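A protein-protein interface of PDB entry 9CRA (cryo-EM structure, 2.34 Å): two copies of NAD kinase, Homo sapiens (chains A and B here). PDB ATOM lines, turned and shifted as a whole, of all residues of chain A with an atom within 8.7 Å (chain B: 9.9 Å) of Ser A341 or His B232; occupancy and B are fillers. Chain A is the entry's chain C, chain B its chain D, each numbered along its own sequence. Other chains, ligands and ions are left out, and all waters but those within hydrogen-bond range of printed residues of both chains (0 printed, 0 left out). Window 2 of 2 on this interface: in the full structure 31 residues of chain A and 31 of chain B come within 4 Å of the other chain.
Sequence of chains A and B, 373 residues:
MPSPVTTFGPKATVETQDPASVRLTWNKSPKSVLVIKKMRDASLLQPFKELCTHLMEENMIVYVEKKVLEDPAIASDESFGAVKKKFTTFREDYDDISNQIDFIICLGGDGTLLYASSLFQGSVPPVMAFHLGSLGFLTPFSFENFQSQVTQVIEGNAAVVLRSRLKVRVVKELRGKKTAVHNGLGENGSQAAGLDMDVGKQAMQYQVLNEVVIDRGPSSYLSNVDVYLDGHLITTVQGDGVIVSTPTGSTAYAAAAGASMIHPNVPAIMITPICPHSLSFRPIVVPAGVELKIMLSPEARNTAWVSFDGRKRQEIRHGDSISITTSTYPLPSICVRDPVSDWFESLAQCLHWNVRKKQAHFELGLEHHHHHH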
ATOM      1  N   PRO A 140      12.486  -5.051  24.204  1.00  0.00           N
ATOM      2  CA  PRO A 140      12.260  -3.792  24.921  1.00  0.00           C
ATOM      3  C   PRO A 140      10.918  -3.652  25.624  1.00  0.00           C
ATOM      4  O   PRO A 140      10.737  -2.671  26.358  1.00  0.00           O
ATOM      5  CB  PRO A 140      12.376  -2.760  23.794  1.00  0.00           C
ATOM      6  CG  PRO A 140      11.796  -3.470  22.616  1.00  0.00           C
ATOM      7  CD  PRO A 140      12.140  -4.937  22.778  1.00  0.00           C
ATOM      8  N   VAL A 161      12.496  -0.409  13.938  1.00  0.00           N
ATOM      9  CA  VAL A 161      13.914  -0.374  13.600  1.00  0.00           C
ATOM     10  C   VAL A 161      14.172  -1.491  12.601  1.00  0.00           C
ATOM     11  O   VAL A 161      13.969  -2.670  12.915  1.00  0.00           O
ATOM     12  CB  VAL A 161      14.805  -0.536  14.841  1.00  0.00           C
ATOM     13  CG1 VAL A 161      16.270  -0.398  14.465  1.00  0.00           C
ATOM     14  CG2 VAL A 161      14.422   0.476  15.907  1.00  0.00           C
ATOM     15  N   HIS A 263      25.193   1.221  16.178  1.00  0.00           N
ATOM     16  CA  HIS A 263      23.744   1.355  16.198  1.00  0.00           C
ATOM     17  C   HIS A 263      23.132   0.588  15.028  1.00  0.00           C
ATOM     18  O   HIS A 263      23.695   0.579  13.928  1.00  0.00           O
ATOM     19  CB  HIS A 263      23.362   2.836  16.129  1.00  0.00           C
ATOM     20  CG  HIS A 263      21.934   3.121  16.480  1.00  0.00           C
ATOM     21  ND1 HIS A 263      20.883   2.796  15.651  1.00  0.00           N
ATOM     22  CD2 HIS A 263      21.385   3.705  17.571  1.00  0.00           C
ATOM     23  CE1 HIS A 263      19.747   3.165  16.216  1.00  0.00           C
ATOM     24  NE2 HIS A 263      20.025   3.720  17.382  1.00  0.00           N
ATOM     25  N   CYS A 335       9.857  -0.624  18.420  1.00  0.00           N
ATOM     26  CA  CYS A 335      10.509  -0.002  19.562  1.00  0.00           C
ATOM     27  C   CYS A 335       9.474   0.656  20.465  1.00  0.00           C
ATOM     28  O   CYS A 335       8.412   1.089  20.008  1.00  0.00           O
ATOM     29  CB  CYS A 335      11.534   1.033  19.098  1.00  0.00           C
ATOM     30  SG  CYS A 335      10.822   2.441  18.225  1.00  0.00           S
ATOM     31  N   VAL A 336       9.789   0.723  21.761  1.00  0.00           N
ATOM     32  CA  VAL A 336       8.827   1.255  22.721  1.00  0.00           C
ATOM     33  C   VAL A 336       8.618   2.752  22.506  1.00  0.00           C
ATOM     34  O   VAL A 336       7.478   3.223  22.412  1.00  0.00           O
ATOM     35  CB  VAL A 336       9.260   0.936  24.165  1.00  0.00           C
ATOM     36  CG1 VAL A 336       9.031  -0.536  24.467  1.00  0.00           C
ATOM     37  CG2 VAL A 336      10.715   1.290  24.395  1.00  0.00           C
ATOM     38  N   ARG A 337       9.702   3.523  22.425  1.00  0.00           N
ATOM     39  CA  ARG A 337       9.578   4.952  22.159  1.00  0.00           C
ATOM     40  C   ARG A 337      10.335   5.413  20.923  1.00  0.00           C
ATOM     41  O   ARG A 337       9.752   6.103  20.077  1.00  0.00           O
ATOM     42  CB  ARG A 337       9.997   5.758  23.405  1.00  0.00           C
ATOM     43  CG  ARG A 337      11.430   5.599  23.875  1.00  0.00           C
ATOM     44  CD  ARG A 337      11.614   6.353  25.183  1.00  0.00           C
ATOM     45  NE  ARG A 337      12.983   6.312  25.681  1.00  0.00           N
ATOM     46  CZ  ARG A 337      13.465   5.355  26.462  1.00  0.00           C
ATOM     47  NH1 ARG A 337      12.719   4.331  26.842  1.00  0.00           N
ATOM     48  NH2 ARG A 337      14.727   5.429  26.875  1.00  0.00           N
ATOM     49  N   ASP A 338      11.603   5.047  20.774  1.00  0.00           N
ATOM     50  CA  ASP A 338      12.385   5.412  19.598  1.00  0.00           C
ATOM     51  C   ASP A 338      13.662   4.566  19.577  1.00  0.00           C
ATOM     52  O   ASP A 338      14.032   3.981  20.598  1.00  0.00           O
ATOM     53  CB  ASP A 338      12.690   6.927  19.568  1.00  0.00           C
ATOM     54  CG  ASP A 338      13.687   7.373  20.627  1.00  0.00           C
ATOM     55  OD1 ASP A 338      14.213   6.540  21.384  1.00  0.00           O
ATOM     56  OD2 ASP A 338      13.917   8.596  20.726  1.00  0.00           O
ATOM     57  N   PRO A 339      14.325   4.465  18.419  1.00  0.00           N
ATOM     58  CA  PRO A 339      15.498   3.571  18.333  1.00  0.00           C
ATOM     59  C   PRO A 339      16.649   3.949  19.253  1.00  0.00           C
ATOM     60  O   PRO A 339      17.196   3.078  19.943  1.00  0.00           O
ATOM     61  CB  PRO A 339      15.899   3.674  16.856  1.00  0.00           C
ATOM     62  CG  PRO A 339      14.666   4.082  16.150  1.00  0.00           C
ATOM     63  CD  PRO A 339      13.911   4.958  17.093  1.00  0.00           C
ATOM     64  N   VAL A 340      17.039   5.225  19.276  1.00  0.00           N
ATOM     65  CA  VAL A 340      18.275   5.618  19.949  1.00  0.00           C
ATOM     66  C   VAL A 340      18.168   5.408  21.454  1.00  0.00           C
ATOM     67  O   VAL A 340      19.073   4.846  22.085  1.00  0.00           O
ATOM     68  CB  VAL A 340      18.626   7.078  19.613  1.00  0.00           C
ATOM     69  CG1 VAL A 340      19.919   7.469  20.298  1.00  0.00           C
ATOM     70  CG2 VAL A 340      18.736   7.266  18.109  1.00  0.00           C
ATOM     71  N   SER A 341      17.074   5.876  22.056  1.00  0.00           N
ATOM     72  CA  SER A 341      16.932   5.756  23.503  1.00  0.00           C
ATOM     73  C   SER A 341      16.821   4.299  23.927  1.00  0.00           C
ATOM     74  O   SER A 341      17.364   3.910  24.964  1.00  0.00           O
ATOM     75  CB  SER A 341      15.724   6.555  23.988  1.00  0.00           C
ATOM     76  OG  SER A 341      15.700   7.846  23.406  1.00  0.00           O
ATOM     77  N   ASP A 342      16.120   3.478  23.141  1.00  0.00           N
ATOM     78  CA  ASP A 342      16.045   2.055  23.451  1.00  0.00           C
ATOM     79  C   ASP A 342      17.415   1.395  23.359  1.00  0.00           C
ATOM     80  O   ASP A 342      17.777   0.578  24.213  1.00  0.00           O
ATOM     81  CB  ASP A 342      15.056   1.360  22.517  1.00  0.00           C
ATOM     82  CG  ASP A 342      13.650   1.888  22.669  1.00  0.00           C
ATOM     83  OD1 ASP A 342      13.441   2.794  23.503  1.00  0.00           O
ATOM     84  OD2 ASP A 342      12.752   1.398  21.955  1.00  0.00           O
ATOM     85  N   TRP A 343      18.195   1.745  22.332  1.00  0.00           N
ATOM     86  CA  TRP A 343      19.536   1.186  22.201  1.00  0.00           C
ATOM     87  C   TRP A 343      20.413   1.572  23.385  1.00  0.00           C
ATOM     88  O   TRP A 343      21.138   0.732  23.934  1.00  0.00           O
ATOM     89  CB  TRP A 343      20.170   1.653  20.890  1.00  0.00           C
ATOM     90  CG  TRP A 343      21.428   0.924  20.533  1.00  0.00           C
ATOM     91  CD1 TRP A 343      21.555  -0.406  20.265  1.00  0.00           C
ATOM     92  CD2 TRP A 343      22.739   1.487  20.404  1.00  0.00           C
ATOM     93  NE1 TRP A 343      22.864  -0.707  19.977  1.00  0.00           N
ATOM     94  CE2 TRP A 343      23.610   0.438  20.056  1.00  0.00           C
ATOM     95  CE3 TRP A 343      23.258   2.777  20.550  1.00  0.00           C
ATOM     96  CZ2 TRP A 343      24.973   0.638  19.852  1.00  0.00           C
ATOM     97  CZ3 TRP A 343      24.609   2.973  20.345  1.00  0.00           C
ATOM     98  CH2 TRP A 343      25.451   1.910  20.001  1.00  0.00           C
ATOM     99  N   PHE A 344      20.349   2.836  23.805  1.00  0.00           N
ATOM    100  CA  PHE A 344      21.193   3.269  24.913  1.00  0.00           C
ATOM    101  C   PHE A 344      20.719   2.700  26.246  1.00  0.00           C
ATOM    102  O   PHE A 344      21.545   2.395  27.113  1.00  0.00           O
ATOM    103  CB  PHE A 344      21.264   4.794  24.960  1.00  0.00           C
ATOM    104  CG  PHE A 344      22.308   5.370  24.049  1.00  0.00           C
ATOM    105  CD1 PHE A 344      23.624   5.484  24.465  1.00  0.00           C
ATOM    106  CD2 PHE A 344      21.979   5.789  22.772  1.00  0.00           C
ATOM    107  CE1 PHE A 344      24.587   6.008  23.627  1.00  0.00           C
ATOM    108  CE2 PHE A 344      22.939   6.314  21.931  1.00  0.00           C
ATOM    109  CZ  PHE A 344      24.244   6.424  22.359  1.00  0.00           C
ATOM    110  N   GLU A 345      19.406   2.533  26.429  1.00  0.00           N
ATOM    111  CA  GLU A 345      18.915   1.853  27.622  1.00  0.00           C
ATOM    112  C   GLU A 345      19.362   0.400  27.649  1.00  0.00           C
ATOM    113  O   GLU A 345      19.705  -0.130  28.710  1.00  0.00           O
ATOM    114  CB  GLU A 345      17.392   1.944  27.705  1.00  0.00           C
ATOM    115  CG  GLU A 345      16.883   3.223  28.344  1.00  0.00           C
ATOM    116  CD  GLU A 345      15.478   3.076  28.893  1.00  0.00           C
ATOM    117  OE1 GLU A 345      15.130   1.965  29.347  1.00  0.00           O
ATOM    118  OE2 GLU A 345      14.723   4.071  28.882  1.00  0.00           O
ATOM    119  N   SER A 346      19.355  -0.267  26.493  1.00  0.00           N
ATOM    120  CA  SER A 346      19.862  -1.633  26.432  1.00  0.00           C
ATOM    121  C   SER A 346      21.341  -1.682  26.790  1.00  0.00           C
ATOM    122  O   SER A 346      21.778  -2.568  27.533  1.00  0.00           O
ATOM    123  CB  SER A 346      19.623  -2.219  25.041  1.00  0.00           C
ATOM    124  OG  SER A 346      18.238  -2.322  24.763  1.00  0.00           O
ATOM    125  N   LEU A 347      22.125  -0.730  26.278  1.00  0.00           N
ATOM    126  CA  LEU A 347      23.542  -0.671  26.632  1.00  0.00           C
ATOM    127  C   LEU A 347      23.731  -0.456  28.130  1.00  0.00           C
ATOM    128  O   LEU A 347      24.596  -1.086  28.750  1.00  0.00           O
ATOM    129  CB  LEU A 347      24.240   0.439  25.847  1.00  0.00           C
ATOM    130  CG  LEU A 347      24.426   0.251  24.341  1.00  0.00           C
ATOM    131  CD1 LEU A 347      24.989   1.516  23.719  1.00  0.00           C
ATOM    132  CD2 LEU A 347      25.342  -0.926  24.069  1.00  0.00           C
ATOM    133  N   ALA A 348      22.934   0.433  28.727  1.00  0.00           N
ATOM    134  CA  ALA A 348      23.108   0.753  30.140  1.00  0.00           C
ATOM    135  C   ALA A 348      22.632  -0.373  31.051  1.00  0.00           C
ATOM    136  O   ALA A 348      23.205  -0.577  32.127  1.00  0.00           O
ATOM    137  CB  ALA A 348      22.373   2.050  30.478  1.00  0.00           C
ATOM    138  N   GLN A 349      21.596  -1.108  30.648  1.00  0.00           N
ATOM    139  CA  GLN A 349      20.989  -2.100  31.526  1.00  0.00           C
ATOM    140  C   GLN A 349      21.576  -3.494  31.346  1.00  0.00           C
ATOM    141  O   GLN A 349      21.769  -4.212  32.331  1.00  0.00           O
ATOM    142  CB  GLN A 349      19.476  -2.143  31.293  1.00  0.00           C
ATOM    143  CG  GLN A 349      18.687  -1.187  32.170  1.00  0.00           C
ATOM    144  CD  GLN A 349      17.188  -1.330  31.987  1.00  0.00           C
ATOM    145  OE1 GLN A 349      16.726  -1.999  31.064  1.00  0.00           O
ATOM    146  NE2 GLN A 349      16.422  -0.701  32.870  1.00  0.00           N
ATOM    147  N   ASP B 226      29.868  16.032  29.465  1.00  0.00           N
ATOM    148  CA  ASP B 226      28.563  15.458  29.169  1.00  0.00           C
ATOM    149  C   ASP B 226      28.336  15.474  27.663  1.00  0.00           C
ATOM    150  O   ASP B 226      28.569  16.499  27.009  1.00  0.00           O
ATOM    151  CB  ASP B 226      27.455  16.245  29.868  1.00  0.00           C
ATOM    152  CG  ASP B 226      27.226  15.792  31.294  1.00  0.00           C
ATOM    153  OD1 ASP B 226      28.165  15.238  31.899  1.00  0.00           O
ATOM    154  OD2 ASP B 226      26.106  15.991  31.810  1.00  0.00           O
ATOM    155  N   VAL B 227      27.881  14.348  27.109  1.00  0.00           N
ATOM    156  CA  VAL B 227      27.593  14.261  25.682  1.00  0.00           C
ATOM    157  C   VAL B 227      26.120  13.922  25.495  1.00  0.00           C
ATOM    158  O   VAL B 227      25.591  13.015  26.148  1.00  0.00           O
ATOM    159  CB  VAL B 227      28.509  13.246  24.968  1.00  0.00           C
ATOM    160  CG1 VAL B 227      28.330  11.855  25.523  1.00  0.00           C
ATOM    161  CG2 VAL B 227      28.249  13.260  23.469  1.00  0.00           C
ATOM    162  N   TYR B 228      25.455  14.682  24.629  1.00  0.00           N
ATOM    163  CA  TYR B 228      24.048  14.517  24.306  1.00  0.00           C
ATOM    164  C   TYR B 228      23.926  14.077  22.854  1.00  0.00           C
ATOM    165  O   TYR B 228      24.674  14.549  21.992  1.00  0.00           O
ATOM    166  CB  TYR B 228      23.274  15.828  24.489  1.00  0.00           C
ATOM    167  CG  TYR B 228      23.239  16.388  25.894  1.00  0.00           C
ATOM    168  CD1 TYR B 228      23.658  15.636  26.982  1.00  0.00           C
ATOM    169  CD2 TYR B 228      22.777  17.675  26.130  1.00  0.00           C
ATOM    170  CE1 TYR B 228      23.623  16.153  28.262  1.00  0.00           C
ATOM    171  CE2 TYR B 228      22.736  18.199  27.405  1.00  0.00           C
ATOM    172  CZ  TYR B 228      23.159  17.434  28.468  1.00  0.00           C
ATOM    173  OH  TYR B 228      23.122  17.954  29.742  1.00  0.00           O
ATOM    174  N   LEU B 229      22.982  13.184  22.577  1.00  0.00           N
ATOM    175  CA  LEU B 229      22.669  12.794  21.208  1.00  0.00           C
ATOM    176  C   LEU B 229      21.192  13.067  20.973  1.00  0.00           C
ATOM    177  O   LEU B 229      20.336  12.467  21.630  1.00  0.00           O
ATOM    178  CB  LEU B 229      23.010  11.323  20.954  1.00  0.00           C
ATOM    179  CG  LEU B 229      22.918  10.791  19.518  1.00  0.00           C
ATOM    180  CD1 LEU B 229      23.866   9.614  19.342  1.00  0.00           C
ATOM    181  CD2 LEU B 229      21.506  10.396  19.114  1.00  0.00           C
ATOM    182  N   ASP B 230      20.902  13.970  20.035  1.00  0.00           N
ATOM    183  CA  ASP B 230      19.532  14.368  19.707  1.00  0.00           C
ATOM    184  C   ASP B 230      18.795  14.902  20.933  1.00  0.00           C
ATOM    185  O   ASP B 230      17.613  14.625  21.141  1.00  0.00           O
ATOM    186  CB  ASP B 230      18.759  13.215  19.065  1.00  0.00           C
ATOM    187  CG  ASP B 230      18.910  13.182  17.557  1.00  0.00           C
ATOM    188  OD1 ASP B 230      19.125  14.255  16.956  1.00  0.00           O
ATOM    189  OD2 ASP B 230      18.810  12.083  16.972  1.00  0.00           O
ATOM    190  N   GLY B 231      19.501  15.678  21.754  1.00  0.00           N
ATOM    191  CA  GLY B 231      18.897  16.314  22.906  1.00  0.00           C
ATOM    192  C   GLY B 231      18.747  15.441  24.130  1.00  0.00           C
ATOM    193  O   GLY B 231      18.151  15.888  25.116  1.00  0.00           O
ATOM    194  N   HIS B 232      19.268  14.218  24.108  1.00  0.00           N
ATOM    195  CA  HIS B 232      19.148  13.288  25.221  1.00  0.00           C
ATOM    196  C   HIS B 232      20.536  12.964  25.750  1.00  0.00           C
ATOM    197  O   HIS B 232      21.451  12.685  24.970  1.00  0.00           O
ATOM    198  CB  HIS B 232      18.435  12.004  24.788  1.00  0.00           C
ATOM    199  CG  HIS B 232      16.957  12.163  24.613  1.00  0.00           C
ATOM    200  ND1 HIS B 232      16.207  11.317  23.825  1.00  0.00           N
ATOM    201  CD2 HIS B 232      16.091  13.072  25.119  1.00  0.00           C
ATOM    202  CE1 HIS B 232      14.943  11.697  23.854  1.00  0.00           C
ATOM    203  NE2 HIS B 232      14.845  12.759  24.633  1.00  0.00           N
ATOM    204  N   LEU B 233      20.688  12.995  27.071  1.00  0.00           N
ATOM    205  CA  LEU B 233      21.971  12.685  27.686  1.00  0.00           C
ATOM    206  C   LEU B 233      22.246  11.194  27.555  1.00  0.00           C
ATOM    207  O   LEU B 233      21.507  10.370  28.102  1.00  0.00           O
ATOM    208  CB  LEU B 233      21.975  13.114  29.153  1.00  0.00           C
ATOM    209  CG  LEU B 233      23.276  13.050  29.963  1.00  0.00           C
ATOM    210  CD1 LEU B 233      23.236  14.073  31.084  1.00  0.00           C
ATOM    211  CD2 LEU B 233      23.526  11.664  30.544  1.00  0.00           C
ATOM    212  N   ILE B 234      23.308  10.845  26.835  1.00  0.00           N
ATOM    213  CA  ILE B 234      23.668   9.453  26.623  1.00  0.00           C
ATOM    214  C   ILE B 234      24.747   8.995  27.597  1.00  0.00           C
ATOM    215  O   ILE B 234      24.703   7.857  28.068  1.00  0.00           O
ATOM    216  CB  ILE B 234      24.083   9.210  25.155  1.00  0.00           C
ATOM    217  CG1 ILE B 234      25.457   9.809  24.851  1.00  0.00           C
ATOM    218  CG2 ILE B 234      23.030   9.762  24.211  1.00  0.00           C
ATOM    219  CD1 ILE B 234      25.869   9.694  23.400  1.00  0.00           C
ATOM    220  N   THR B 235      25.704   9.860  27.931  1.00  0.00           N
ATOM    221  CA  THR B 235      26.708   9.518  28.932  1.00  0.00           C
ATOM    222  C   THR B 235      27.517  10.754  29.307  1.00  0.00           C
ATOM    223  O   THR B 235      27.434  11.813  28.670  1.00  0.00           O
ATOM    224  CB  THR B 235      27.646   8.400  28.457  1.00  0.00           C
ATOM    225  OG1 THR B 235      28.459   7.961  29.552  1.00  0.00           O
ATOM    226  CG2 THR B 235      28.546   8.882  27.340  1.00  0.00           C
ATOM    227  N   THR B 236      28.286  10.596  30.382  1.00  0.00           N
ATOM    228  CA  THR B 236      29.277  11.559  30.835  1.00  0.00           C
ATOM    229  C   THR B 236      30.625  10.856  30.857  1.00  0.00           C
ATOM    230  O   THR B 236      30.804   9.872  31.581  1.00  0.00           O
ATOM    231  CB  THR B 236      28.935  12.095  32.227  1.00  0.00           C
ATOM    232  OG1 THR B 236      27.806  12.974  32.141  1.00  0.00           O
ATOM    233  CG2 THR B 236      30.118  12.847  32.817  1.00  0.00           C
ATOM    234  N   ILE B 271      32.400   7.711  18.330  1.00  0.00           N
ATOM    235  CA  ILE B 271      32.680   8.325  19.623  1.00  0.00           C
ATOM    236  C   ILE B 271      33.644   7.407  20.359  1.00  0.00           C
ATOM    237  O   ILE B 271      33.292   6.268  20.690  1.00  0.00           O
ATOM    238  CB  ILE B 271      31.407   8.563  20.450  1.00  0.00           C
ATOM    239  CG1 ILE B 271      30.457   9.504  19.706  1.00  0.00           C
ATOM    240  CG2 ILE B 271      31.759   9.136  21.812  1.00  0.00           C
ATOM    241  CD1 ILE B 271      29.000   9.279  20.022  1.00  0.00           C
ATOM    242  N   PRO B 287      24.606   6.694  13.760  1.00  0.00           N
ATOM    243  CA  PRO B 287      24.269   7.114  12.395  1.00  0.00           C
ATOM    244  C   PRO B 287      24.745   8.529  12.107  1.00  0.00           C
ATOM    245  O   PRO B 287      24.849   9.369  13.002  1.00  0.00           O
ATOM    246  CB  PRO B 287      22.739   7.022  12.365  1.00  0.00           C
ATOM    247  CG  PRO B 287      22.405   6.034  13.421  1.00  0.00           C
ATOM    248  CD  PRO B 287      23.415   6.247  14.504  1.00  0.00           C
ATOM    249  N   VAL B 290      22.554  12.190  12.911  1.00  0.00           N
ATOM    250  CA  VAL B 290      22.140  12.531  14.261  1.00  0.00           C
ATOM    251  C   VAL B 290      22.796  13.838  14.688  1.00  0.00           C
ATOM    252  O   VAL B 290      23.769  14.309  14.094  1.00  0.00           O
ATOM    253  CB  VAL B 290      22.463  11.404  15.267  1.00  0.00           C
ATOM    254  CG1 VAL B 290      21.759  10.115  14.873  1.00  0.00           C
ATOM    255  CG2 VAL B 290      23.960  11.199  15.371  1.00  0.00           C
ATOM    256  N   GLU B 291      22.244  14.430  15.743  1.00  0.00           N
ATOM    257  CA  GLU B 291      22.773  15.634  16.367  1.00  0.00           C
ATOM    258  C   GLU B 291      23.634  15.242  17.559  1.00  0.00           C
ATOM    259  O   GLU B 291      23.182  14.494  18.432  1.00  0.00           O
ATOM    260  CB  GLU B 291      21.633  16.543  16.833  1.00  0.00           C
ATOM    261  CG  GLU B 291      22.070  17.857  17.468  1.00  0.00           C
ATOM    262  CD  GLU B 291      22.774  18.779  16.500  1.00  0.00           C
ATOM    263  OE1 GLU B 291      22.512  18.666  15.286  1.00  0.00           O
ATOM    264  OE2 GLU B 291      23.587  19.613  16.949  1.00  0.00           O
ATOM    265  N   LEU B 292      24.867  15.740  17.599  1.00  0.00           N
ATOM    266  CA  LEU B 292      25.723  15.553  18.762  1.00  0.00           C
ATOM    267  C   LEU B 292      25.952  16.887  19.456  1.00  0.00           C
ATOM    268  O   LEU B 292      26.161  17.910  18.802  1.00  0.00           O
ATOM    269  CB  LEU B 292      27.064  14.923  18.381  1.00  0.00           C
ATOM    270  CG  LEU B 292      27.165  13.416  18.628  1.00  0.00           C
ATOM    271  CD1 LEU B 292      26.219  12.655  17.723  1.00  0.00           C
ATOM    272  CD2 LEU B 292      28.588  12.937  18.437  1.00  0.00           C
ATOM    273  N   LYS B 293      25.904  16.871  20.783  1.00  0.00           N
ATOM    274  CA  LYS B 293      26.182  18.048  21.588  1.00  0.00           C
ATOM    275  C   LYS B 293      27.131  17.654  22.707  1.00  0.00           C
ATOM    276  O   LYS B 293      27.084  16.535  23.215  1.00  0.00           O
ATOM    277  CB  LYS B 293      24.891  18.650  22.157  1.00  0.00           C
ATOM    278  CG  LYS B 293      24.971  20.135  22.462  1.00  0.00           C
ATOM    279  CD  LYS B 293      23.961  20.532  23.522  1.00  0.00           C
ATOM    280  CE  LYS B 293      24.161  21.971  23.957  1.00  0.00           C
ATOM    281  NZ  LYS B 293      23.800  22.929  22.876  1.00  0.00           N
ATOM    282  N   ILE B 294      28.008  18.579  23.077  1.00  0.00           N
ATOM    283  CA  ILE B 294      29.034  18.316  24.079  1.00  0.00           C
ATOM    284  C   ILE B 294      29.159  19.541  24.971  1.00  0.00           C
ATOM    285  O   ILE B 294      29.331  20.663  24.476  1.00  0.00           O
ATOM    286  CB  ILE B 294      30.384  17.959  23.429  1.00  0.00           C
ATOM    287  CG1 ILE B 294      30.385  16.488  23.005  1.00  0.00           C
ATOM    288  CG2 ILE B 294      31.535  18.254  24.371  1.00  0.00           C
ATOM    289  CD1 ILE B 294      31.635  16.050  22.291  1.00  0.00           C
ATOM    290  N   MET B 295      29.049  19.329  26.283  1.00  0.00           N
ATOM    291  CA  MET B 295      29.145  20.408  27.255  1.00  0.00           C
ATOM    292  C   MET B 295      29.955  19.940  28.453  1.00  0.00           C
ATOM    293  O   MET B 295      30.304  18.764  28.583  1.00  0.00           O
ATOM    294  CB  MET B 295      27.764  20.886  27.729  1.00  0.00           C
ATOM    295  CG  MET B 295      26.713  21.035  26.645  1.00  0.00           C
ATOM    296  SD  MET B 295      25.093  21.410  27.339  1.00  0.00           S
ATOM    297  CE  MET B 295      25.310  23.128  27.791  1.00  0.00           C
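The side-chain carboxylate (OD1) of Asp A338 lies within hydrogen-bond range of the side-chain hydroxyl (OG) of Ser A341, at 2.8 Å.
O of Val B227 lies within hydrogen-bond range of N of Ile B234 (3.2 Å).
Pro B287 touches His A263.
Val A340 touches Leu B229 (CG1 to CD2, 3.5 Å).
OG of Ser A341 touches ND1 of His B232, at 3.5 Å.
Ile B234 touches Phe A344 (CB to CE1, 3.6 Å).
Ser A341 touches just one residue of chain B: His B232.
His B232 touches just one residue of chain A: Ser A341 (3.5 Å).
No residue of chain B comes within 4 Å of Asp A338.
Val A340 touches just one residue of chain B: Leu B229 (3.5 Å).
No residue of chain B comes within 4 Å of Asp A342.
No residue of chain A comes within 4 Å of Gly B231.
Of the printed residues of chain B, Phe A344 touches Ile B234 (3.6 Å).
Of the printed residues of chain A, Leu B229 touches Val A340.
Cys A335 touches none of the printed residues of chain B.
Gln A349 touches none of the printed residues of chain B.
The nearest residue of chain A that does not touch His B232 is Asp A338 (4.5 Å).
Of the 19 printed residues of chain B, 4 touch a printed residue of chain A.
Printed residues of chain B that touch a printed residue of chain A: Leu B229, His B232, Ile B234 and Pro B287.
Hydrophobic or aromatic side chains of chain B within 4 Å of the printed part of chain A: Leu B229, His B232, Ile B234 and Pro B287.
Of the 18 printed residues of chain A, 4 touch a printed residue of chain B.
Hydrophobic or aromatic side chains of chain A that line the printed part of chain B: His A263, Val A340 and Phe A344.
No position is printed for both chains.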
